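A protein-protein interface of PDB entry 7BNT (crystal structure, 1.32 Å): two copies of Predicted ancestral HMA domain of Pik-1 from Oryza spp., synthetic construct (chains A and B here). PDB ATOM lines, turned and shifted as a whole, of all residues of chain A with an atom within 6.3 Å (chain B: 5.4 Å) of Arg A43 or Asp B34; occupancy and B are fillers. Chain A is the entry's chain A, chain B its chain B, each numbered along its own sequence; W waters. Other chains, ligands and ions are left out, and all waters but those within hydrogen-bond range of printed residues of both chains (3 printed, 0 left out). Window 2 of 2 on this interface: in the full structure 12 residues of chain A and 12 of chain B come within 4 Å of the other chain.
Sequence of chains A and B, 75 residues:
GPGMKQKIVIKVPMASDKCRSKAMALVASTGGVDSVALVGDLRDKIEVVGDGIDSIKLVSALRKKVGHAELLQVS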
ATOM      1  N   VAL A  12       9.016   3.426  21.646  1.00  0.00           N
ATOM      2  CA  VAL A  12       8.057   4.468  22.114  1.00  0.00           C
ATOM      3  C   VAL A  12       8.607   5.766  21.564  1.00  0.00           C
ATOM      4  O   VAL A  12       9.628   6.246  22.055  1.00  0.00           O
ATOM      5  CB  VAL A  12       7.955   4.490  23.653  1.00  0.00           C
ATOM      6  CG1 VAL A  12       6.998   5.573  24.134  1.00  0.00           C
ATOM      7  CG2 VAL A  12       7.556   3.138  24.207  1.00  0.00           C
ATOM      8  N   MET A  14       9.529   9.355  21.289  1.00  0.00           N
ATOM      9  CA  MET A  14       9.713  10.281  22.423  1.00  0.00           C
ATOM     10  C   MET A  14       9.732  11.708  21.903  1.00  0.00           C
ATOM     11  O   MET A  14      10.538  11.997  21.015  1.00  0.00           O
ATOM     12  CB  MET A  14      11.028  10.005  23.161  1.00  0.00           C
ATOM     13  CG  MET A  14      11.161   8.575  23.670  1.00  0.00           C
ATOM     14  SD  MET A  14       9.960   8.189  24.945  1.00  0.00           S
ATOM     15  CE  MET A  14      10.504   6.523  25.340  1.00  0.00           C
ATOM     16  N   ASP A  17      12.334  14.340  27.134  1.00  0.00           N
ATOM     17  CA  ASP A  17      12.713  13.559  28.332  1.00  0.00           C
ATOM     18  C   ASP A  17      11.509  13.335  29.256  1.00  0.00           C
ATOM     19  O   ASP A  17      11.530  12.336  29.962  1.00  0.00           O
ATOM     20  CB  ASP A  17      13.869  14.229  29.066  1.00  0.00           C
ATOM     21  CG  ASP A  17      15.211  14.035  28.387  1.00  0.00           C
ATOM     22  OD1 ASP A  17      15.316  13.175  27.462  1.00  0.00           O
ATOM     23  OD2 ASP A  17      16.147  14.745  28.787  1.00  0.00           O
ATOM     24  N   ARG A  20      10.166  10.154  28.027  1.00  0.00           N
ATOM     25  CA  ARG A  20      11.040   9.026  28.414  1.00  0.00           C
ATOM     26  C   ARG A  20      10.757   8.663  29.865  1.00  0.00           C
ATOM     27  O   ARG A  20      10.698   7.466  30.184  1.00  0.00           O
ATOM     28  CB  ARG A  20      12.507   9.371  28.198  1.00  0.00           C
ATOM     29  CG  ARG A  20      12.891   9.511  26.736  1.00  0.00           C
ATOM     30  CD  ARG A  20      14.351   9.875  26.499  1.00  0.00           C
ATOM     31  NE  ARG A  20      14.534  10.038  25.072  1.00  0.00           N
ATOM     32  CZ  ARG A  20      14.315  11.162  24.400  1.00  0.00           C
ATOM     33  NH1 ARG A  20      14.056  12.299  25.034  1.00  0.00           N
ATOM     34  NH2 ARG A  20      14.391  11.135  23.078  1.00  0.00           N
ATOM     35  N   MET A  24       9.349   5.067  31.004  1.00  0.00           N
ATOM     36  CA  MET A  24      10.183   4.229  31.882  1.00  0.00           C
ATOM     37  C   MET A  24       9.444   3.948  33.188  1.00  0.00           C
ATOM     38  O   MET A  24       9.487   2.801  33.660  1.00  0.00           O
ATOM     39  CB  MET A  24      11.528   4.906  32.143  1.00  0.00           C
ATOM     40  CG  MET A  24      12.450   4.781  30.964  1.00  0.00           C
ATOM     41  SD  MET A  24      13.035   3.074  30.708  1.00  0.00           S
ATOM     42  CE  MET A  24      14.343   3.001  31.938  1.00  0.00           C
ATOM     43  N   VAL A  36      14.594  -3.065  33.403  1.00  0.00           N
ATOM     44  CA  VAL A  36      14.179  -2.140  32.321  1.00  0.00           C
ATOM     45  C   VAL A  36      15.410  -1.414  31.834  1.00  0.00           C
ATOM     46  O   VAL A  36      16.126  -0.857  32.664  1.00  0.00           O
ATOM     47  CB  VAL A  36      13.098  -1.162  32.792  1.00  0.00           C
ATOM     48  CG1 VAL A  36      12.577  -0.402  31.616  1.00  0.00           C
ATOM     49  CG2 VAL A  36      11.973  -1.854  33.544  1.00  0.00           C
ATOM     50  N   ALA A  37      15.600  -1.358  30.523  1.00  0.00           N
ATOM     51  CA  ALA A  37      16.715  -0.605  29.931  1.00  0.00           C
ATOM     52  C   ALA A  37      16.161   0.255  28.800  1.00  0.00           C
ATOM     53  O   ALA A  37      15.401  -0.245  27.944  1.00  0.00           O
ATOM     54  CB  ALA A  37      17.824  -1.515  29.447  1.00  0.00           C
ATOM     55  N   LEU A  38      16.582   1.512  28.790  1.00  0.00           N
ATOM     56  CA  LEU A  38      16.229   2.465  27.729  1.00  0.00           C
ATOM     57  C   LEU A  38      17.441   2.486  26.808  1.00  0.00           C
ATOM     58  O   LEU A  38      18.547   2.807  27.254  1.00  0.00           O
ATOM     59  CB  LEU A  38      15.900   3.824  28.350  1.00  0.00           C
ATOM     60  CG  LEU A  38      15.330   4.886  27.420  1.00  0.00           C
ATOM     61  CD1 LEU A  38      14.015   4.440  26.828  1.00  0.00           C
ATOM     62  CD2 LEU A  38      15.150   6.193  28.186  1.00  0.00           C
ATOM     63  N   VAL A  39      17.230   2.135  25.543  1.00  0.00           N
ATOM     64  CA  VAL A  39      18.319   1.910  24.567  1.00  0.00           C
ATOM     65  C   VAL A  39      17.990   2.672  23.280  1.00  0.00           C
ATOM     66  O   VAL A  39      16.899   3.252  23.135  1.00  0.00           O
ATOM     67  CB  VAL A  39      18.597   0.416  24.335  1.00  0.00           C
ATOM     68  CG1 VAL A  39      18.846  -0.336  25.639  1.00  0.00           C
ATOM     69  CG2 VAL A  39      17.499  -0.277  23.560  1.00  0.00           C
ATOM     70  N   GLY A  40      18.957   2.706  22.389  1.00  0.00           N
ATOM     71  CA  GLY A  40      18.831   3.424  21.105  1.00  0.00           C
ATOM     72  C   GLY A  40      19.483   4.795  21.162  1.00  0.00           C
ATOM     73  O   GLY A  40      19.540   5.443  22.224  1.00  0.00           O
ATOM     74  N   ASP A  41      19.897   5.292  20.012  1.00  0.00           N
ATOM     75  CA  ASP A  41      20.502   6.637  19.875  1.00  0.00           C
ATOM     76  C   ASP A  41      19.600   7.706  20.500  1.00  0.00           C
ATOM     77  O   ASP A  41      20.140   8.620  21.173  1.00  0.00           O
ATOM     78  CB  ASP A  41      20.745   6.959  18.413  1.00  0.00           C
ATOM     79  CG  ASP A  41      21.805   6.108  17.749  1.00  0.00           C
ATOM     80  OD1 ASP A  41      22.532   5.351  18.458  1.00  0.00           O
ATOM     81  OD2 ASP A  41      21.914   6.233  16.515  1.00  0.00           O
ATOM     82  N   LEU A  42      18.282   7.598  20.289  1.00  0.00           N
ATOM     83  CA  LEU A  42      17.291   8.582  20.788  1.00  0.00           C
ATOM     84  C   LEU A  42      16.630   8.078  22.067  1.00  0.00           C
ATOM     85  O   LEU A  42      15.617   8.677  22.500  1.00  0.00           O
ATOM     86  CB  LEU A  42      16.272   8.896  19.690  1.00  0.00           C
ATOM     87  CG  LEU A  42      16.733   9.868  18.607  1.00  0.00           C
ATOM     88  CD1 LEU A  42      15.754   9.805  17.447  1.00  0.00           C
ATOM     89  CD2 LEU A  42      16.845  11.294  19.150  1.00  0.00           C
ATOM     90  N   ARG A  43      17.203   7.057  22.699  1.00  0.00           N
ATOM     91  CA  ARG A  43      16.716   6.585  24.009  1.00  0.00           C
ATOM     92  C   ARG A  43      15.200   6.441  23.911  1.00  0.00           C
ATOM     93  O   ARG A  43      14.460   7.057  24.709  1.00  0.00           O
ATOM     94  CB  ARG A  43      17.179   7.528  25.123  1.00  0.00           C
ATOM     95  CG  ARG A  43      18.690   7.478  25.290  1.00  0.00           C
ATOM     96  CD  ARG A  43      19.193   8.482  26.286  1.00  0.00           C
ATOM     97  NE  ARG A  43      19.020   7.950  27.621  1.00  0.00           N
ATOM     98  CZ  ARG A  43      18.246   8.477  28.542  1.00  0.00           C
ATOM     99  NH1 ARG A  43      17.539   9.560  28.271  1.00  0.00           N
ATOM    100  NH2 ARG A  43      18.181   7.919  29.739  1.00  0.00           N
ATOM    101  N   ASP A  44      14.761   5.600  22.987  1.00  0.00           N
ATOM    102  CA  ASP A  44      13.320   5.478  22.661  1.00  0.00           C
ATOM    103  C   ASP A  44      12.933   4.015  22.438  1.00  0.00           C
ATOM    104  O   ASP A  44      11.785   3.788  22.026  1.00  0.00           O
ATOM    105  CB  ASP A  44      12.978   6.325  21.440  1.00  0.00           C
ATOM    106  CG  ASP A  44      13.689   5.925  20.164  1.00  0.00           C
ATOM    107  OD1 ASP A  44      14.525   5.000  20.206  1.00  0.00           O
ATOM    108  OD2 ASP A  44      13.383   6.556  19.125  1.00  0.00           O
ATOM    109  N   LYS A  45      13.786   3.071  22.828  1.00  0.00           N
ATOM    110  CA  LYS A  45      13.471   1.628  22.833  1.00  0.00           C
ATOM    111  C   LYS A  45      13.629   1.117  24.246  1.00  0.00           C
ATOM    112  O   LYS A  45      14.681   1.346  24.878  1.00  0.00           O
ATOM    113  CB  LYS A  45      14.367   0.867  21.859  1.00  0.00           C
ATOM    114  CG  LYS A  45      14.006   1.088  20.405  1.00  0.00           C
ATOM    115  CD  LYS A  45      14.998   0.459  19.473  1.00  0.00           C
ATOM    116  CE  LYS A  45      16.079   1.428  19.049  1.00  0.00           C
ATOM    117  NZ  LYS A  45      16.831   0.922  17.879  1.00  0.00           N
ATOM    118  N   LYS B   5      29.641   5.918  32.724  1.00  0.00           N
ATOM    119  CA  LYS B   5      28.379   5.621  33.438  1.00  0.00           C
ATOM    120  C   LYS B   5      28.682   5.302  34.906  1.00  0.00           C
ATOM    121  O   LYS B   5      29.749   4.808  35.232  1.00  0.00           O
ATOM    122  CB  LYS B   5      27.646   4.455  32.780  1.00  0.00           C
ATOM    123  CG  LYS B   5      27.325   4.652  31.300  1.00  0.00           C
ATOM    124  CD  LYS B   5      26.314   5.726  31.058  1.00  0.00           C
ATOM    125  CE  LYS B   5      25.957   5.836  29.583  1.00  0.00           C
ATOM    126  NZ  LYS B   5      24.854   6.784  29.358  1.00  0.00           N
ATOM    127  N   GLY B  32      18.618  10.928  33.494  1.00  0.00           N
ATOM    128  CA  GLY B  32      19.959  10.352  33.277  1.00  0.00           C
ATOM    129  C   GLY B  32      20.049   8.878  33.608  1.00  0.00           C
ATOM    130  O   GLY B  32      21.137   8.363  33.581  1.00  0.00           O
ATOM    131  N   VAL B  33      18.950   8.242  33.968  1.00  0.00           N
ATOM    132  CA  VAL B  33      18.910   6.773  34.177  1.00  0.00           C
ATOM    133  C   VAL B  33      18.806   6.073  32.830  1.00  0.00           C
ATOM    134  O   VAL B  33      17.930   6.400  32.031  1.00  0.00           O
ATOM    135  CB  VAL B  33      17.777   6.378  35.134  1.00  0.00           C
ATOM    136  CG1 VAL B  33      17.570   4.863  35.171  1.00  0.00           C
ATOM    137  CG2 VAL B  33      18.059   6.960  36.513  1.00  0.00           C
ATOM    138  N   ASP B  34      19.671   5.106  32.605  1.00  0.00           N
ATOM    139  CA  ASP B  34      19.652   4.235  31.416  1.00  0.00           C
ATOM    140  C   ASP B  34      18.951   2.920  31.727  1.00  0.00           C
ATOM    141  O   ASP B  34      18.255   2.418  30.831  1.00  0.00           O
ATOM    142  CB  ASP B  34      21.056   3.982  30.919  1.00  0.00           C
ATOM    143  CG  ASP B  34      21.739   5.259  30.473  1.00  0.00           C
ATOM    144  OD1 ASP B  34      21.026   6.190  30.039  1.00  0.00           O
ATOM    145  OD2 ASP B  34      22.941   5.300  30.647  1.00  0.00           O
ATOM    146  N   SER B  35      19.159   2.354  32.902  1.00  0.00           N
ATOM    147  CA  SER B  35      18.610   1.020  33.179  1.00  0.00           C
ATOM    148  C   SER B  35      18.486   0.820  34.681  1.00  0.00           C
ATOM    149  O   SER B  35      19.267   1.392  35.456  1.00  0.00           O
ATOM    150  CB  SER B  35      19.407  -0.088  32.513  1.00  0.00           C
ATOM    151  OG  SER B  35      20.777   0.027  32.834  1.00  0.00           O
ATOM    152  N   VAL B  36      17.545  -0.056  35.030  1.00  0.00           N
ATOM    153  CA  VAL B  36      17.287  -0.411  36.446  1.00  0.00           C
ATOM    154  C   VAL B  36      17.049  -1.913  36.483  1.00  0.00           C
ATOM    155  O   VAL B  36      16.437  -2.457  35.562  1.00  0.00           O
ATOM    156  CB  VAL B  36      16.070   0.317  37.049  1.00  0.00           C
ATOM    157  CG1 VAL B  36      16.328   1.798  37.109  1.00  0.00           C
ATOM    158  CG2 VAL B  36      14.793   0.026  36.299  1.00  0.00           C
ATOM    159  N   VAL B  49      21.896   2.278  36.563  1.00  0.00           N
ATOM    160  CA  VAL B  49      23.036   2.672  35.711  1.00  0.00           C
ATOM    161  C   VAL B  49      22.610   3.901  34.915  1.00  0.00           C
ATOM    162  O   VAL B  49      21.496   3.954  34.369  1.00  0.00           O
ATOM    163  CB  VAL B  49      23.487   1.522  34.809  1.00  0.00           C
ATOM    164  CG1 VAL B  49      24.467   1.962  33.738  1.00  0.00           C
ATOM    165  CG2 VAL B  49      24.078   0.427  35.655  1.00  0.00           C
ATOM    166  N   GLY B  50      23.495   4.866  34.854  1.00  0.00           N
ATOM    167  CA  GLY B  50      23.244   6.042  34.041  1.00  0.00           C
ATOM    168  C   GLY B  50      24.322   7.063  34.244  1.00  0.00           C
ATOM    169  O   GLY B  50      25.395   6.729  34.644  1.00  0.00           O
ATOM    170  N   ASP B  51      24.035   8.285  33.899  1.00  0.00           N
ATOM    171  CA  ASP B  51      25.047   9.335  34.106  1.00  0.00           C
ATOM    172  C   ASP B  51      24.359  10.558  34.695  1.00  0.00           C
ATOM    173  O   ASP B  51      23.168  10.773  34.476  1.00  0.00           O
ATOM    174  CB  ASP B  51      25.847   9.520  32.825  1.00  0.00           C
ATOM    175  CG  ASP B  51      24.971   9.880  31.664  1.00  0.00           C
ATOM    176  OD1 ASP B  51      24.349  10.942  31.755  1.00  0.00           O
ATOM    177  OD2 ASP B  51      24.906   9.095  30.690  1.00  0.00           O
HETATM  178  O   HOH W   1      20.280   4.941  27.250  1.00  0.00           O
HETATM  179  O   HOH W   2      22.241   7.777  28.285  1.00  0.00           O
HETATM  180  O   HOH W   3      17.080  11.460  30.944  1.00  0.00           O
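The backbone carbonyl oxygen of Val A36 lies within hydrogen-bond range of the backbone NH of Val B36 (2.9 Å).
O of Asp B34 sits at hydrogen-bond distance from N of Leu A38 (2.8 Å).
The guanidinium group (NH2) of Arg A43 sits at hydrogen-bond distance from the backbone carbonyl oxygen (O) of Val B33.
NH2 of Arg A43 lies within salt-bridge range of OD1 of Asp B34, 3.3 Å away.
NE of Arg A20 lies within hydrogen-bond range of O of Arg A43, 3.0 Å away.
OD2 of Asp B34 lies within salt-bridge range of NZ of Lys B5, 2.7 Å away.
The backbone NH (N) of Asp B34 sits at hydrogen-bond distance from the backbone carbonyl oxygen (O) of Val B49 (2.8 Å).
O of Ser B35 sits at hydrogen-bond distance from N of Val B49 (3.0 Å).
Ser B35 touches Val A36.
CA of Ala A37 touches O of Asp B34 (3.5 Å).
CB of Ser B35 touches CB of Ala A37, at 3.7 Å.
Arg A43 touches just these residues of chain B: Val B33 (2.8 Å) and Asp B34 (3.3 Å).
Asp B34 touches just these residues of chain A: Ala A37, Leu A38 and Arg A43.
Of the printed residues of chain B, Ala A37 touches Asp B34 and Ser B35.
Printed residues of chain B within 4 Å of Leu A38: Asp B34 (2.8 Å).
Of the printed residues of chain A, Val B36 touches Val A36 (2.9 Å).
Of the printed residues of chain A, Val B33 touches Arg A43 (2.8 Å).
Arg A20 touches none of the printed residues of chain B.
The nearest residue of chain B that does not touch Arg A43 is Gly B32 (4.4 Å).
The nearest printed residue of chain A that does not touch Val B33 is Leu A38 (4.7 Å).
Hydrophobic or aromatic side chains of chain B that line the printed part of chain A: Val B36.
Among the printed residues, 7 pairs touch across the chains.
Among the printed residues, Asp or Glu carboxylates within 4 Å of a Lys or Arg side-chain nitrogen of the other chain: Arg A43 with Asp B34 (3.3 Å).
Val B36 touches its own counterpart, Val A36.
Water W2 lies within hydrogen-bond range of the side-chain carboxylate (OD1) of Asp B34 (2.7 Å), the side-chain amino group (NZ) of Lys B5 (3.0 Å) and the guanidinium group (NE) of Arg A43 (3.3 Å).
Water W1 lies within hydrogen-bond range of O of Leu A38, OD1 of Asp B34 and NE of Arg A43.
Water W3 lies within hydrogen-bond range of N of Gly B32 and NH1 of Arg A43.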
